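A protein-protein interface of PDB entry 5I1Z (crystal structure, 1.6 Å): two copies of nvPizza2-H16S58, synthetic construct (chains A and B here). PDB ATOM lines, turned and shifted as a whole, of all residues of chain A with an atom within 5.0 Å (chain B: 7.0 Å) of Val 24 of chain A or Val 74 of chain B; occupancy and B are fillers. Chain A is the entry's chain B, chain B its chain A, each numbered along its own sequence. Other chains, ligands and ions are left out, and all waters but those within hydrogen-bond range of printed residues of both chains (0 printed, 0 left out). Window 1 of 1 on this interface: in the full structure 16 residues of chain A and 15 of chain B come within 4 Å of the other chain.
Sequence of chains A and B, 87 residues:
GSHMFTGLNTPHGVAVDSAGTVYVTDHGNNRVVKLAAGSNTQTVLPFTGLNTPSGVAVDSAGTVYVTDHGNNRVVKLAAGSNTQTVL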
ATOM      1  N   PHE A   5      -1.228  27.547  -0.607  1.00  0.00           N
ATOM      2  CA  PHE A   5      -1.101  26.096  -0.411  1.00  0.00           C
ATOM      3  C   PHE A   5      -0.671  25.534  -1.750  1.00  0.00           C
ATOM      4  O   PHE A   5      -1.163  25.970  -2.793  1.00  0.00           O
ATOM      5  CB  PHE A   5      -2.377  25.450   0.096  1.00  0.00           C
ATOM      6  CG  PHE A   5      -2.665  25.728   1.550  1.00  0.00           C
ATOM      7  CD1 PHE A   5      -1.731  25.417   2.549  1.00  0.00           C
ATOM      8  CD2 PHE A   5      -3.847  26.366   1.919  1.00  0.00           C
ATOM      9  CE1 PHE A   5      -1.997  25.661   3.876  1.00  0.00           C
ATOM     10  CE2 PHE A   5      -4.076  26.654   3.232  1.00  0.00           C
ATOM     11  CZ  PHE A   5      -3.166  26.289   4.213  1.00  0.00           C
ATOM     12  N   LEU A   8      -1.828  20.456  -2.601  1.00  0.00           N
ATOM     13  CA  LEU A   8      -2.784  19.818  -1.718  1.00  0.00           C
ATOM     14  C   LEU A   8      -3.593  18.852  -2.492  1.00  0.00           C
ATOM     15  O   LEU A   8      -3.951  19.129  -3.651  1.00  0.00           O
ATOM     16  CB  LEU A   8      -3.809  20.818  -1.133  1.00  0.00           C
ATOM     17  CG  LEU A   8      -3.513  21.719   0.022  1.00  0.00           C
ATOM     18  CD1 LEU A   8      -4.854  22.365   0.397  1.00  0.00           C
ATOM     19  CD2 LEU A   8      -2.882  20.952   1.164  1.00  0.00           C
ATOM     20  N   PRO A  11      -7.994  17.433   0.754  1.00  0.00           N
ATOM     21  CA  PRO A  11      -7.851  17.805   2.182  1.00  0.00           C
ATOM     22  C   PRO A  11      -9.051  17.382   3.010  1.00  0.00           C
ATOM     23  O   PRO A  11     -10.174  17.479   2.551  1.00  0.00           O
ATOM     24  CB  PRO A  11      -7.775  19.341   2.114  1.00  0.00           C
ATOM     25  CG  PRO A  11      -8.588  19.718   0.885  1.00  0.00           C
ATOM     26  CD  PRO A  11      -8.193  18.632  -0.093  1.00  0.00           C
ATOM     27  N   GLY A  13      -9.403  18.275   6.573  1.00  0.00           N
ATOM     28  CA  GLY A  13      -9.684  19.018   7.823  1.00  0.00           C
ATOM     29  C   GLY A  13      -8.939  20.325   7.871  1.00  0.00           C
ATOM     30  O   GLY A  13      -7.905  20.451   7.269  1.00  0.00           O
ATOM     31  N   VAL A  14      -9.493  21.305   8.633  1.00  0.00           N
ATOM     32  CA  VAL A  14      -8.834  22.583   8.781  1.00  0.00           C
ATOM     33  C   VAL A  14      -8.933  23.087  10.223  1.00  0.00           C
ATOM     34  O   VAL A  14      -9.953  22.854  10.859  1.00  0.00           O
ATOM     35  CB  VAL A  14      -9.375  23.595   7.752  1.00  0.00           C
ATOM     36  CG1 VAL A  14     -10.905  23.771   7.880  1.00  0.00           C
ATOM     37  CG2 VAL A  14      -8.616  24.918   7.850  1.00  0.00           C
ATOM     38  N   VAL A  22      -3.320  28.913   9.638  1.00  0.00           N
ATOM     39  CA  VAL A  22      -4.271  27.852   9.158  1.00  0.00           C
ATOM     40  C   VAL A  22      -3.509  26.543   9.042  1.00  0.00           C
ATOM     41  O   VAL A  22      -2.415  26.527   8.432  1.00  0.00           O
ATOM     42  CB  VAL A  22      -4.857  28.231   7.828  1.00  0.00           C
ATOM     43  CG1 VAL A  22      -5.814  27.160   7.261  1.00  0.00           C
ATOM     44  CG2 VAL A  22      -5.600  29.601   7.866  1.00  0.00           C
ATOM     45  N   TYR A  23      -4.099  25.465   9.542  1.00  0.00           N
ATOM     46  CA  TYR A  23      -3.477  24.123   9.582  1.00  0.00           C
ATOM     47  C   TYR A  23      -4.432  23.181   8.821  1.00  0.00           C
ATOM     48  O   TYR A  23      -5.629  23.216   9.043  1.00  0.00           O
ATOM     49  CB  TYR A  23      -3.312  23.589  10.979  1.00  0.00           C
ATOM     50  CG  TYR A  23      -2.487  24.473  11.857  1.00  0.00           C
ATOM     51  CD1 TYR A  23      -3.021  25.647  12.394  1.00  0.00           C
ATOM     52  CD2 TYR A  23      -1.196  24.130  12.159  1.00  0.00           C
ATOM     53  CE1 TYR A  23      -2.282  26.446  13.236  1.00  0.00           C
ATOM     54  CE2 TYR A  23      -0.407  24.989  12.960  1.00  0.00           C
ATOM     55  CZ  TYR A  23      -0.959  26.105  13.515  1.00  0.00           C
ATOM     56  OH  TYR A  23      -0.225  26.974  14.374  1.00  0.00           O
ATOM     57  N   VAL A  24      -3.896  22.414   7.881  1.00  0.00           N
ATOM     58  CA  VAL A  24      -4.725  21.612   6.987  1.00  0.00           C
ATOM     59  C   VAL A  24      -4.159  20.169   6.905  1.00  0.00           C
ATOM     60  O   VAL A  24      -2.918  19.972   6.705  1.00  0.00           O
ATOM     61  CB  VAL A  24      -4.748  22.198   5.567  1.00  0.00           C
ATOM     62  CG1 VAL A  24      -5.478  21.318   4.591  1.00  0.00           C
ATOM     63  CG2 VAL A  24      -5.428  23.538   5.571  1.00  0.00           C
ATOM     64  N   THR A  25      -5.051  19.206   6.985  1.00  0.00           N
ATOM     65  CA  THR A  25      -4.689  17.795   6.712  1.00  0.00           C
ATOM     66  C   THR A  25      -4.819  17.495   5.193  1.00  0.00           C
ATOM     67  O   THR A  25      -5.880  17.565   4.570  1.00  0.00           O
ATOM     68  CB  THR A  25      -5.499  16.810   7.540  1.00  0.00           C
ATOM     69  OG1 THR A  25      -6.871  17.011   7.238  1.00  0.00           O
ATOM     70  CG2 THR A  25      -5.263  16.998   8.992  1.00  0.00           C
ATOM     71  N   ASP A  26      -3.651  17.179   4.629  1.00  0.00           N
ATOM     72  CA  ASP A  26      -3.457  16.933   3.167  1.00  0.00           C
ATOM     73  C   ASP A  26      -3.509  15.474   3.060  1.00  0.00           C
ATOM     74  O   ASP A  26      -2.495  14.732   3.050  1.00  0.00           O
ATOM     75  CB  ASP A  26      -2.143  17.527   2.707  1.00  0.00           C
ATOM     76  CG  ASP A  26      -1.957  17.453   1.188  1.00  0.00           C
ATOM     77  OD1 ASP A  26      -2.948  17.077   0.567  1.00  0.00           O
ATOM     78  OD2 ASP A  26      -0.861  17.827   0.654  1.00  0.00           O
ATOM     79  N   ARG A  31       0.181  14.257   4.839  1.00  0.00           N
ATOM     80  CA  ARG A  31       0.923  15.243   5.603  1.00  0.00           C
ATOM     81  C   ARG A  31      -0.025  16.314   6.107  1.00  0.00           C
ATOM     82  O   ARG A  31      -1.192  16.383   5.728  1.00  0.00           O
ATOM     83  CB  ARG A  31       1.968  15.855   4.720  1.00  0.00           C
ATOM     84  CG  ARG A  31       1.469  16.640   3.568  1.00  0.00           C
ATOM     85  CD  ARG A  31       2.587  17.166   2.645  1.00  0.00           C
ATOM     86  NE  ARG A  31       1.955  17.984   1.662  1.00  0.00           N
ATOM     87  CZ  ARG A  31       2.516  18.799   0.786  1.00  0.00           C
ATOM     88  NH1 ARG A  31       3.815  18.981   0.737  1.00  0.00           N
ATOM     89  NH2 ARG A  31       1.728  19.477  -0.010  1.00  0.00           N
ATOM     90  N   VAL A  32       0.580  17.141   6.939  1.00  0.00           N
ATOM     91  CA  VAL A  32      -0.121  18.286   7.550  1.00  0.00           C
ATOM     92  C   VAL A  32       0.670  19.521   7.227  1.00  0.00           C
ATOM     93  O   VAL A  32       1.894  19.564   7.415  1.00  0.00           O
ATOM     94  CB  VAL A  32      -0.304  18.126   9.073  1.00  0.00           C
ATOM     95  CG1 VAL A  32      -1.151  19.276   9.587  1.00  0.00           C
ATOM     96  CG2 VAL A  32      -0.916  16.762   9.442  1.00  0.00           C
ATOM     97  N   VAL A  33      -0.001  20.518   6.665  1.00  0.00           N
ATOM     98  CA  VAL A  33       0.613  21.763   6.265  1.00  0.00           C
ATOM     99  C   VAL A  33       0.046  22.950   7.019  1.00  0.00           C
ATOM    100  O   VAL A  33      -1.160  22.951   7.447  1.00  0.00           O
ATOM    101  CB  VAL A  33       0.468  21.974   4.775  1.00  0.00           C
ATOM    102  CG1 VAL A  33       1.084  20.793   3.998  1.00  0.00           C
ATOM    103  CG2 VAL A  33      -0.946  22.061   4.324  1.00  0.00           C
ATOM    104  N   VAL A  56      -7.840  17.898  12.409  1.00  0.00           N
ATOM    105  CA  VAL A  56      -6.784  18.699  12.989  1.00  0.00           C
ATOM    106  C   VAL A  56      -7.423  19.695  13.971  1.00  0.00           C
ATOM    107  O   VAL A  56      -8.512  20.244  13.746  1.00  0.00           O
ATOM    108  CB  VAL A  56      -5.885  19.342  11.887  1.00  0.00           C
ATOM    109  CG1 VAL A  56      -6.613  20.245  10.919  1.00  0.00           C
ATOM    110  CG2 VAL A  56      -4.657  20.013  12.518  1.00  0.00           C
ATOM    111  N   TYR B  65     -13.264  29.181   7.399  1.00  0.00           N
ATOM    112  CA  TYR B  65     -12.318  28.472   6.522  1.00  0.00           C
ATOM    113  C   TYR B  65     -12.941  27.105   6.210  1.00  0.00           C
ATOM    114  O   TYR B  65     -13.429  26.469   7.104  1.00  0.00           O
ATOM    115  CB  TYR B  65     -11.010  28.256   7.257  1.00  0.00           C
ATOM    116  CG  TYR B  65     -10.386  29.529   7.785  1.00  0.00           C
ATOM    117  CD1 TYR B  65     -10.861  30.084   8.951  1.00  0.00           C
ATOM    118  CD2 TYR B  65      -9.320  30.070   7.173  1.00  0.00           C
ATOM    119  CE1 TYR B  65     -10.298  31.262   9.468  1.00  0.00           C
ATOM    120  CE2 TYR B  65      -8.715  31.250   7.708  1.00  0.00           C
ATOM    121  CZ  TYR B  65      -9.219  31.786   8.817  1.00  0.00           C
ATOM    122  OH  TYR B  65      -8.589  32.969   9.283  1.00  0.00           O
ATOM    123  N   VAL B  66     -12.796  26.670   4.955  1.00  0.00           N
ATOM    124  CA  VAL B  66     -13.396  25.408   4.466  1.00  0.00           C
ATOM    125  C   VAL B  66     -12.372  24.664   3.640  1.00  0.00           C
ATOM    126  O   VAL B  66     -11.799  25.204   2.685  1.00  0.00           O
ATOM    127  CB  VAL B  66     -14.669  25.719   3.671  1.00  0.00           C
ATOM    128  CG1 VAL B  66     -15.261  24.400   3.101  1.00  0.00           C
ATOM    129  CG2 VAL B  66     -15.706  26.390   4.597  1.00  0.00           C
ATOM    130  N   THR B  67     -12.272  23.362   3.895  1.00  0.00           N
ATOM    131  CA  THR B  67     -11.542  22.447   3.012  1.00  0.00           C
ATOM    132  C   THR B  67     -12.484  21.926   1.934  1.00  0.00           C
ATOM    133  O   THR B  67     -13.521  21.230   2.181  1.00  0.00           O
ATOM    134  CB  THR B  67     -10.926  21.293   3.747  1.00  0.00           C
ATOM    135  OG1 THR B  67     -11.815  20.795   4.738  1.00  0.00           O
ATOM    136  CG2 THR B  67      -9.783  21.730   4.641  1.00  0.00           C
ATOM    137  N   ASP B  68     -12.093  22.258   0.703  1.00  0.00           N
ATOM    138  CA  ASP B  68     -12.902  22.000  -0.467  1.00  0.00           C
ATOM    139  C   ASP B  68     -12.364  20.704  -1.045  1.00  0.00           C
ATOM    140  O   ASP B  68     -11.490  20.723  -1.913  1.00  0.00           O
ATOM    141  CB  ASP B  68     -12.861  23.194  -1.467  1.00  0.00           C
ATOM    142  CG  ASP B  68     -13.787  22.976  -2.655  1.00  0.00           C
ATOM    143  OD1 ASP B  68     -14.539  21.983  -2.581  1.00  0.00           O
ATOM    144  OD2 ASP B  68     -13.857  23.816  -3.561  1.00  0.00           O
ATOM    145  N   ASN B  71     -11.946  19.732  -4.816  1.00  0.00           N
ATOM    146  CA  ASN B  71     -11.123  20.670  -5.563  1.00  0.00           C
ATOM    147  C   ASN B  71      -9.730  20.954  -5.000  1.00  0.00           C
ATOM    148  O   ASN B  71      -9.055  21.906  -5.459  1.00  0.00           O
ATOM    149  CB  ASN B  71     -11.915  21.964  -5.717  1.00  0.00           C
ATOM    150  CG  ASN B  71     -13.151  21.772  -6.549  1.00  0.00           C
ATOM    151  OD1 ASN B  71     -13.131  21.108  -7.617  1.00  0.00           O
ATOM    152  ND2 ASN B  71     -14.258  22.362  -6.082  1.00  0.00           N
ATOM    153  N   ASN B  72      -9.278  20.145  -4.027  1.00  0.00           N
ATOM    154  CA  ASN B  72      -7.883  20.144  -3.588  1.00  0.00           C
ATOM    155  C   ASN B  72      -7.467  21.532  -3.186  1.00  0.00           C
ATOM    156  O   ASN B  72      -6.368  21.996  -3.509  1.00  0.00           O
ATOM    157  CB  ASN B  72      -6.971  19.620  -4.690  1.00  0.00           C
ATOM    158  CG  ASN B  72      -7.346  18.256  -5.121  1.00  0.00           C
ATOM    159  OD1 ASN B  72      -7.623  17.369  -4.318  1.00  0.00           O
ATOM    160  ND2 ASN B  72      -7.476  18.090  -6.451  1.00  0.00           N
ATOM    161  N   ARG B  73      -8.342  22.216  -2.431  1.00  0.00           N
ATOM    162  CA  ARG B  73      -8.096  23.614  -2.019  1.00  0.00           C
ATOM    163  C   ARG B  73      -8.757  23.965  -0.693  1.00  0.00           C
ATOM    164  O   ARG B  73      -9.653  23.246  -0.223  1.00  0.00           O
ATOM    165  CB  ARG B  73      -8.485  24.585  -3.113  1.00  0.00           C
ATOM    166  CG  ARG B  73      -9.967  24.695  -3.282  1.00  0.00           C
ATOM    167  CD  ARG B  73     -10.420  25.549  -4.444  1.00  0.00           C
ATOM    168  NE  ARG B  73     -11.853  25.611  -4.461  1.00  0.00           N
ATOM    169  CZ  ARG B  73     -12.536  26.516  -5.105  1.00  0.00           C
ATOM    170  NH1 ARG B  73     -11.886  27.442  -5.801  1.00  0.00           N
ATOM    171  NH2 ARG B  73     -13.850  26.494  -5.035  1.00  0.00           N
ATOM    172  N   VAL B  74      -8.354  25.103  -0.118  1.00  0.00           N
ATOM    173  CA  VAL B  74      -8.923  25.652   1.134  1.00  0.00           C
ATOM    174  C   VAL B  74      -9.382  27.031   0.767  1.00  0.00           C
ATOM    175  O   VAL B  74      -8.651  27.736   0.073  1.00  0.00           O
ATOM    176  CB  VAL B  74      -7.876  25.747   2.236  1.00  0.00           C
ATOM    177  CG1 VAL B  74      -8.472  26.236   3.560  1.00  0.00           C
ATOM    178  CG2 VAL B  74      -7.258  24.385   2.379  1.00  0.00           C
ATOM    179  N   VAL B  75     -10.618  27.347   1.146  1.00  0.00           N
ATOM    180  CA  VAL B  75     -11.205  28.635   0.874  1.00  0.00           C
ATOM    181  C   VAL B  75     -11.602  29.336   2.177  1.00  0.00           C
ATOM    182  O   VAL B  75     -11.779  28.685   3.226  1.00  0.00           O
ATOM    183  CB  VAL B  75     -12.392  28.489  -0.080  1.00  0.00           C
ATOM    184  CG1 VAL B  75     -11.878  28.022  -1.419  1.00  0.00           C
ATOM    185  CG2 VAL B  75     -13.496  27.537   0.440  1.00  0.00           C
ATOM    186  N   LYS B  76     -11.611  30.672   2.120  1.00  0.00           N
ATOM    187  CA  LYS B  76     -12.040  31.448   3.292  1.00  0.00           C
ATOM    188  C   LYS B  76     -12.952  32.609   2.916  1.00  0.00           C
ATOM    189  O   LYS B  76     -12.952  33.095   1.756  1.00  0.00           O
ATOM    190  CB  LYS B  76     -10.918  31.948   4.162  1.00  0.00           C
ATOM    191  CG  LYS B  76     -10.161  33.121   3.577  1.00  0.00           C
ATOM    192  CD  LYS B  76      -9.106  33.610   4.538  1.00  0.00           C
ATOM    193  CE  LYS B  76      -8.268  34.590   3.764  1.00  0.00           C
ATOM    194  NZ  LYS B  76      -7.152  35.135   4.564  1.00  0.00           N
ATOM    195  N   THR B  85     -11.725  33.858  -0.692  1.00  0.00           N
ATOM    196  CA  THR B  85     -10.303  33.845  -1.035  1.00  0.00           C
ATOM    197  C   THR B  85      -9.871  32.379  -1.053  1.00  0.00           C
ATOM    198  O   THR B  85     -10.060  31.656  -0.035  1.00  0.00           O
ATOM    199  CB  THR B  85      -9.441  34.553   0.012  1.00  0.00           C
ATOM    200  OG1 THR B  85      -9.792  35.922   0.052  1.00  0.00           O
ATOM    201  CG2 THR B  85      -7.926  34.471  -0.331  1.00  0.00           C
ATOM    202  N   VAL B  86      -9.204  31.939  -2.128  1.00  0.00           N
ATOM    203  CA  VAL B  86      -8.514  30.637  -2.090  1.00  0.00           C
ATOM    204  C   VAL B  86      -7.129  30.776  -1.410  1.00  0.00           C
ATOM    205  O   VAL B  86      -6.305  31.608  -1.826  1.00  0.00           O
ATOM    206  CB  VAL B  86      -8.392  30.024  -3.537  1.00  0.00           C
ATOM    207  CG1 VAL B  86      -7.757  28.642  -3.504  1.00  0.00           C
ATOM    208  CG2 VAL B  86      -9.717  29.993  -4.238  1.00  0.00           C
ATOM    209  N   LEU B  87      -6.845  29.976  -0.390  1.00  0.00           N
ATOM    210  CA  LEU B  87      -5.590  30.064   0.333  1.00  0.00           C
ATOM    211  C   LEU B  87      -4.482  29.366  -0.403  1.00  0.00           C
ATOM    212  O   LEU B  87      -4.666  28.504  -1.303  1.00  0.00           O
ATOM    213  CB  LEU B  87      -5.664  29.497   1.748  1.00  0.00           C
ATOM    214  CG  LEU B  87      -6.517  30.254   2.802  1.00  0.00           C
ATOM    215  CD1 LEU B  87      -8.003  30.127   2.470  1.00  0.00           C
ATOM    216  CD2 LEU B  87      -6.220  29.593   4.117  1.00  0.00           C
ATOM    217  OXT LEU B  87      -3.335  29.732  -0.073  1.00  0.00           O
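OXT of Leu 87 of chain B sits at hydrogen-bond distance from N of Phe 5 of chain A (3.1 Å).
The side-chain carboxylate (OD2) of Asp 68 of chain B is in salt-bridge range of the guanidinium group (NE) of Arg 73 of chain B (2.8 Å). The backbone NH of Leu 87 of chain B is in hydrogen-bond range of the backbone carbonyl oxygen of Val 74 of chain B. N of Gly 13 of chain A sits at hydrogen-bond distance from OG1 of Thr 25 of chain A, 2.9 Å away. The backbone NH (N) of Val 24 of chain A lies within hydrogen-bond range of the backbone carbonyl oxygen (O) of Val 33 of chain A (2.8 Å).
Phe 5 of chain A touches Val 74 of chain B (CD2 to CG2, 3.97 Å). Leu 8 of chain A touches Asn 72 of chain B (O to CB, 3.2 Å). Val 74 of chain B touches Leu 8 of chain A. CD of Pro 11 of chain A touches CA of Asn 72 of chain B (3.8 Å). Gly 13 of chain A touches Thr 67 of chain B. Tyr 65 of chain B touches Val 14 of chain A (O to CG1, 3.8 Å). Val 14 of chain A touches Thr 67 of chain B. Tyr 65 of chain B touches Val 22 of chain A (CE2 to CG2, 3.5 Å). Val 22 of chain A touches Leu 87 of chain B (CG2 to CD2, 3.8 Å). CG2 of Val 24 of chain A touches CG2 of Val 74 of chain B (3.8 Å).
Printed residues of chain B within 4 Å of Pro 11 of chain A: Asn 72 and Arg 73. Printed residues of chain B within 4 Å of Val 14 of chain A: Tyr 65 and Thr 67. Val 24 of chain A touches just one residue of chain B: Val 74 (3.8 Å). Of the printed residues of chain A, Tyr 65 of chain B touches Val 14 and Val 22. Of the printed residues of chain A, Arg 73 of chain B touches Pro 11. Val 74 of chain B touches three residues of chain A. Of the printed residues of chain A, Leu 87 of chain B touches Phe 5 (3.1 Å) and Val 22 (3.8 Å).
Hydrophobic or aromatic side chains of chain A that line the printed part of chain B: Phe 5, Leu 8, Pro 11, Val 14, Val 22 and Val 24. Of the 13 printed residues of chain B, 6 touch a printed residue of chain A. Among the printed residues, 12 pairs touch across the chains. Among the printed residues, no Asp or Glu carboxylate lies within 4 Å of a Lys or Arg side-chain nitrogen of the other chain.
No position is printed for both chains.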
